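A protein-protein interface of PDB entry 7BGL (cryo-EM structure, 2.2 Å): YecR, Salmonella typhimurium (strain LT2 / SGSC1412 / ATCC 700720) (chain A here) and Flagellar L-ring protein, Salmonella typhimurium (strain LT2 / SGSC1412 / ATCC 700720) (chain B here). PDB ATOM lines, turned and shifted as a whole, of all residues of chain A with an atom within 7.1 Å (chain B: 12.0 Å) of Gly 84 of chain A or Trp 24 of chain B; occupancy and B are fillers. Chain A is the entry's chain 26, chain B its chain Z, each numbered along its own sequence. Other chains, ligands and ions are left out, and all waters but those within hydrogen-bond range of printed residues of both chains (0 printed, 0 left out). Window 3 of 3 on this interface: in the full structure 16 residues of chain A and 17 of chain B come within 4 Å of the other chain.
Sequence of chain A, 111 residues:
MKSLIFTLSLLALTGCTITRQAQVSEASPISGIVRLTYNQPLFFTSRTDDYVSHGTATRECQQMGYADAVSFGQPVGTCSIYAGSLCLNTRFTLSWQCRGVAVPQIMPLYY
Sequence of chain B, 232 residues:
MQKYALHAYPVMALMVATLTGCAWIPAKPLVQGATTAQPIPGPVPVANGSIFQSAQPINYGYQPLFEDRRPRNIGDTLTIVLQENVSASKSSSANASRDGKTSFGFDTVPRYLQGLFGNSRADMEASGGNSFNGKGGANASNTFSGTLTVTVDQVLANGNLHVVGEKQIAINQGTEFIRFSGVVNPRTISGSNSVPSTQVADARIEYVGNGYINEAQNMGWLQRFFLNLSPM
N of Ala 27 of chain B lies within hydrogen-bond range of O of Tyr 82 of chain A (2.8 Å).
O of Tyr 82 of chain A touches O of Ile 25 of chain B, 3.5 Å away. Tyr 82 of chain A touches Pro 26 of chain B. Trp 24 of chain B touches Ala 83 of chain A. Ala 23 of chain B touches Gly 84 of chain A. Gly 84 of chain A touches Trp 24 of chain B (CA to CE3, 3.5 Å). CZ3 of Trp 24 of chain B touches N of Ser 85 of chain A, 3.5 Å away. CG of Leu 86 of chain A touches CZ3 of Trp 24 of chain B (3.9 Å). Pro 26 of chain B touches Leu 88 of chain A.
Trp 24 of chain B touches just these residues of chain A: Ala 83 (3.1 Å), Gly 84 (3.5 Å), Ser 85 (3.5 Å) and Leu 86 (3.9 Å). Of chain B, only Ile 25 (3.5 Å), Pro 26 (2.9 Å) and Ala 27 (2.8 Å) come within 4 Å of Tyr 82 of chain A. Ala 83 of chain A touches just one residue of chain B: Trp 24 (3.1 Å). Of chain B, only Trp 24 comes within 4 Å of Leu 86 of chain A. Of the printed residues of chain A, Ala 23 of chain B touches Gly 84. Of the printed residues of chain A, Pro 26 of chain B touches Tyr 82 and Leu 88. Printed residues of chain A within 4 Å of Ile 25 of chain B: Tyr 82. Printed residues of chain A within 4 Å of Ala 27 of chain B: Tyr 82. Of the printed residues of chain B, Leu 88 of chain A touches Pro 26 (3.7 Å). Cys 87 of chain A touches none of the printed residues of chain B. Pro 29 of chain B touches none of the printed residues of chain A. The nearest residue of chain A that does not touch Trp 24 of chain B is Tyr 82 of chain A (5.0 Å). The nearest printed residue of chain A that does not touch Ile 25 of chain B is Ala 83 of chain A (4.3 Å).
Printed residues of chain B that touch a printed residue of chain A: Ala 23, Trp 24, Ile 25, Pro 26 and Ala 27. Hydrophobic or aromatic side chains of chain B that line the printed part of chain A: Trp 24 and Pro 26. Among the printed residues, 9 pairs touch across the chains.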
ATOM      1  N   TYR A  82      14.785  -6.639 -21.811  1.00  0.00           N
ATOM      2  CA  TYR A  82      14.393  -5.252 -22.015  1.00  0.00           C
ATOM      3  C   TYR A  82      14.002  -4.635 -20.682  1.00  0.00           C
ATOM      4  O   TYR A  82      13.210  -5.214 -19.931  1.00  0.00           O
ATOM      5  CB  TYR A  82      13.233  -5.147 -23.008  1.00  0.00           C
ATOM      6  CG  TYR A  82      13.671  -4.951 -24.441  1.00  0.00           C
ATOM      7  CD1 TYR A  82      14.536  -5.848 -25.051  1.00  0.00           C
ATOM      8  CD2 TYR A  82      13.223  -3.866 -25.183  1.00  0.00           C
ATOM      9  CE1 TYR A  82      14.940  -5.673 -26.360  1.00  0.00           C
ATOM     10  CE2 TYR A  82      13.623  -3.682 -26.492  1.00  0.00           C
ATOM     11  CZ  TYR A  82      14.481  -4.589 -27.076  1.00  0.00           C
ATOM     12  OH  TYR A  82      14.882  -4.412 -28.379  1.00  0.00           O
ATOM     13  N   ALA A  83      14.559  -3.458 -20.391  1.00  0.00           N
ATOM     14  CA  ALA A  83      14.232  -2.694 -19.184  1.00  0.00           C
ATOM     15  C   ALA A  83      14.012  -1.249 -19.625  1.00  0.00           C
ATOM     16  O   ALA A  83      14.955  -0.452 -19.670  1.00  0.00           O
ATOM     17  CB  ALA A  83      15.328  -2.809 -18.134  1.00  0.00           C
ATOM     18  N   GLY A  84      12.767  -0.917 -19.946  1.00  0.00           N
ATOM     19  CA  GLY A  84      12.480   0.411 -20.457  1.00  0.00           C
ATOM     20  C   GLY A  84      13.235   0.659 -21.747  1.00  0.00           C
ATOM     21  O   GLY A  84      13.299  -0.200 -22.632  1.00  0.00           O
ATOM     22  N   SER A  85      13.820   1.847 -21.863  1.00  0.00           N
ATOM     23  CA  SER A  85      14.601   2.216 -23.044  1.00  0.00           C
ATOM     24  C   SER A  85      16.066   1.812 -22.888  1.00  0.00           C
ATOM     25  O   SER A  85      16.978   2.627 -23.010  1.00  0.00           O
ATOM     26  CB  SER A  85      14.470   3.711 -23.308  1.00  0.00           C
ATOM     27  OG  SER A  85      13.115   4.077 -23.507  1.00  0.00           O
ATOM     28  N   LEU A  86      16.291   0.529 -22.613  1.00  0.00           N
ATOM     29  CA  LEU A  86      17.634   0.011 -22.402  1.00  0.00           C
ATOM     30  C   LEU A  86      17.694  -1.424 -22.910  1.00  0.00           C
ATOM     31  O   LEU A  86      16.698  -1.984 -23.378  1.00  0.00           O
ATOM     32  CB  LEU A  86      18.031   0.095 -20.926  1.00  0.00           C
ATOM     33  CG  LEU A  86      18.319   1.492 -20.372  1.00  0.00           C
ATOM     34  CD1 LEU A  86      18.816   1.405 -18.938  1.00  0.00           C
ATOM     35  CD2 LEU A  86      19.327   2.218 -21.249  1.00  0.00           C
ATOM     36  N   CYS A  87      18.885  -2.019 -22.815  1.00  0.00           N
ATOM     37  CA  CYS A  87      19.121  -3.407 -23.223  1.00  0.00           C
ATOM     38  C   CYS A  87      20.034  -4.035 -22.171  1.00  0.00           C
ATOM     39  O   CYS A  87      21.260  -3.918 -22.246  1.00  0.00           O
ATOM     40  CB  CYS A  87      19.725  -3.482 -24.619  1.00  0.00           C
ATOM     41  SG  CYS A  87      20.045  -5.161 -25.207  1.00  0.00           S
ATOM     42  N   LEU A  88      19.424  -4.701 -21.189  1.00  0.00           N
ATOM     43  CA  LEU A  88      20.203  -5.281 -20.098  1.00  0.00           C
ATOM     44  C   LEU A  88      21.160  -6.351 -20.606  1.00  0.00           C
ATOM     45  O   LEU A  88      22.324  -6.402 -20.190  1.00  0.00           O
ATOM     46  CB  LEU A  88      19.266  -5.858 -19.037  1.00  0.00           C
ATOM     47  CG  LEU A  88      18.302  -4.866 -18.382  1.00  0.00           C
ATOM     48  CD1 LEU A  88      17.521  -5.537 -17.262  1.00  0.00           C
ATOM     49  CD2 LEU A  88      19.054  -3.651 -17.864  1.00  0.00           C
ATOM     50  N   CYS B  22       5.673  -1.053 -13.065  1.00  0.00           N
ATOM     51  CA  CYS B  22       6.471  -0.070 -13.787  1.00  0.00           C
ATOM     52  C   CYS B  22       6.818  -0.567 -15.185  1.00  0.00           C
ATOM     53  O   CYS B  22       6.814  -1.769 -15.446  1.00  0.00           O
ATOM     54  CB  CYS B  22       7.751   0.257 -13.015  1.00  0.00           C
ATOM     55  SG  CYS B  22       7.479   1.011 -11.394  1.00  0.00           S
ATOM     56  N   ALA B  23       7.117   0.369 -16.083  1.00  0.00           N
ATOM     57  CA  ALA B  23       7.503   0.033 -17.446  1.00  0.00           C
ATOM     58  C   ALA B  23       8.987  -0.277 -17.583  1.00  0.00           C
ATOM     59  O   ALA B  23       9.416  -0.705 -18.660  1.00  0.00           O
ATOM     60  CB  ALA B  23       7.133   1.174 -18.397  1.00  0.00           C
ATOM     61  N   TRP B  24       9.775  -0.072 -16.531  1.00  0.00           N
ATOM     62  CA  TRP B  24      11.207  -0.334 -16.563  1.00  0.00           C
ATOM     63  C   TRP B  24      11.570  -1.715 -16.036  1.00  0.00           C
ATOM     64  O   TRP B  24      12.754  -2.064 -16.023  1.00  0.00           O
ATOM     65  CB  TRP B  24      11.954   0.739 -15.765  1.00  0.00           C
ATOM     66  CG  TRP B  24      12.004   2.057 -16.463  1.00  0.00           C
ATOM     67  CD1 TRP B  24      11.079   3.057 -16.393  1.00  0.00           C
ATOM     68  CD2 TRP B  24      13.030   2.521 -17.347  1.00  0.00           C
ATOM     69  NE1 TRP B  24      11.467   4.116 -17.178  1.00  0.00           N
ATOM     70  CE2 TRP B  24      12.662   3.812 -17.774  1.00  0.00           C
ATOM     71  CE3 TRP B  24      14.225   1.970 -17.819  1.00  0.00           C
ATOM     72  CZ2 TRP B  24      13.446   4.560 -18.649  1.00  0.00           C
ATOM     73  CZ3 TRP B  24      15.002   2.714 -18.686  1.00  0.00           C
ATOM     74  CH2 TRP B  24      14.609   3.995 -19.092  1.00  0.00           C
ATOM     75  N   ILE B  25      10.594  -2.501 -15.605  1.00  0.00           N
ATOM     76  CA  ILE B  25      10.888  -3.857 -15.127  1.00  0.00           C
ATOM     77  C   ILE B  25      11.377  -4.702 -16.294  1.00  0.00           C
ATOM     78  O   ILE B  25      10.809  -4.615 -17.397  1.00  0.00           O
ATOM     79  CB  ILE B  25       9.645  -4.474 -14.482  1.00  0.00           C
ATOM     80  CG1 ILE B  25       9.250  -3.686 -13.231  1.00  0.00           C
ATOM     81  CG2 ILE B  25       9.897  -5.932 -14.136  1.00  0.00           C
ATOM     82  CD1 ILE B  25       8.016  -4.219 -12.542  1.00  0.00           C
ATOM     83  N   PRO B  26      12.415  -5.518 -16.116  1.00  0.00           N
ATOM     84  CA  PRO B  26      12.892  -6.347 -17.229  1.00  0.00           C
ATOM     85  C   PRO B  26      11.793  -7.266 -17.739  1.00  0.00           C
ATOM     86  O   PRO B  26      11.007  -7.816 -16.966  1.00  0.00           O
ATOM     87  CB  PRO B  26      14.050  -7.140 -16.611  1.00  0.00           C
ATOM     88  CG  PRO B  26      14.470  -6.344 -15.418  1.00  0.00           C
ATOM     89  CD  PRO B  26      13.225  -5.694 -14.901  1.00  0.00           C
ATOM     90  N   ALA B  27      11.746  -7.426 -19.059  1.00  0.00           N
ATOM     91  CA  ALA B  27      10.734  -8.259 -19.688  1.00  0.00           C
ATOM     92  C   ALA B  27      11.334  -8.946 -20.904  1.00  0.00           C
ATOM     93  O   ALA B  27      12.277  -8.441 -21.520  1.00  0.00           O
ATOM     94  CB  ALA B  27       9.502  -7.441 -20.094  1.00  0.00           C
ATOM     95  N   LYS B  28      10.775 -10.106 -21.243  1.00  0.00           N
ATOM     96  CA  LYS B  28      11.216 -10.878 -22.395  1.00  0.00           C
ATOM     97  C   LYS B  28      10.162 -10.804 -23.486  1.00  0.00           C
ATOM     98  O   LYS B  28       9.024 -11.248 -23.267  1.00  0.00           O
ATOM     99  CB  LYS B  28      11.477 -12.331 -22.005  1.00  0.00           C
ATOM    100  CG  LYS B  28      12.258 -12.500 -20.715  1.00  0.00           C
ATOM    101  CD  LYS B  28      12.561 -13.963 -20.445  1.00  0.00           C
ATOM    102  CE  LYS B  28      13.753 -14.442 -21.257  1.00  0.00           C
ATOM    103  NZ  LYS B  28      15.008 -13.743 -20.869  1.00  0.00           N
ATOM    104  N   PRO B  29      10.477 -10.261 -24.659  1.00  0.00           N
ATOM    105  CA  PRO B  29       9.486 -10.226 -25.740  1.00  0.00           C
ATOM    106  C   PRO B  29       9.085 -11.632 -26.158  1.00  0.00           C
ATOM    107  O   PRO B  29       9.884 -12.569 -26.109  1.00  0.00           O
ATOM    108  CB  PRO B  29      10.217  -9.489 -26.868  1.00  0.00           C
ATOM    109  CG  PRO B  29      11.666  -9.692 -26.575  1.00  0.00           C
ATOM    110  CD  PRO B  29      11.780  -9.721 -25.081  1.00  0.00           C
ATOM    111  N   GLN B 173       0.756  -3.334 -24.032  1.00  0.00           N
ATOM    112  CA  GLN B 173       0.286  -3.499 -22.661  1.00  0.00           C
ATOM    113  C   GLN B 173      -0.586  -4.750 -22.533  1.00  0.00           C
ATOM    114  O   GLN B 173      -1.772  -4.688 -22.202  1.00  0.00           O
ATOM    115  CB  GLN B 173      -0.469  -2.251 -22.192  1.00  0.00           C
ATOM    116  CG  GLN B 173       0.175  -0.939 -22.612  1.00  0.00           C
ATOM    117  CD  GLN B 173       1.635  -0.857 -22.226  1.00  0.00           C
ATOM    118  OE1 GLN B 173       2.068  -1.480 -21.257  1.00  0.00           O
ATOM    119  NE2 GLN B 173       2.406  -0.086 -22.983  1.00  0.00           N
ATOM    120  N   TYR B 212      -2.999  -5.807 -17.385  1.00  0.00           N
ATOM    121  CA  TYR B 212      -4.026  -5.143 -16.592  1.00  0.00           C
ATOM    122  C   TYR B 212      -5.346  -5.064 -17.345  1.00  0.00           C
ATOM    123  O   TYR B 212      -6.409  -5.000 -16.721  1.00  0.00           O
ATOM    124  CB  TYR B 212      -3.561  -3.748 -16.165  1.00  0.00           C
ATOM    125  CG  TYR B 212      -3.307  -2.776 -17.297  1.00  0.00           C
ATOM    126  CD1 TYR B 212      -4.356  -2.107 -17.911  1.00  0.00           C
ATOM    127  CD2 TYR B 212      -2.017  -2.510 -17.735  1.00  0.00           C
ATOM    128  CE1 TYR B 212      -4.131  -1.213 -18.937  1.00  0.00           C
ATOM    129  CE2 TYR B 212      -1.782  -1.617 -18.760  1.00  0.00           C
ATOM    130  CZ  TYR B 212      -2.842  -0.972 -19.358  1.00  0.00           C
ATOM    131  OH  TYR B 212      -2.614  -0.082 -20.379  1.00  0.00           O
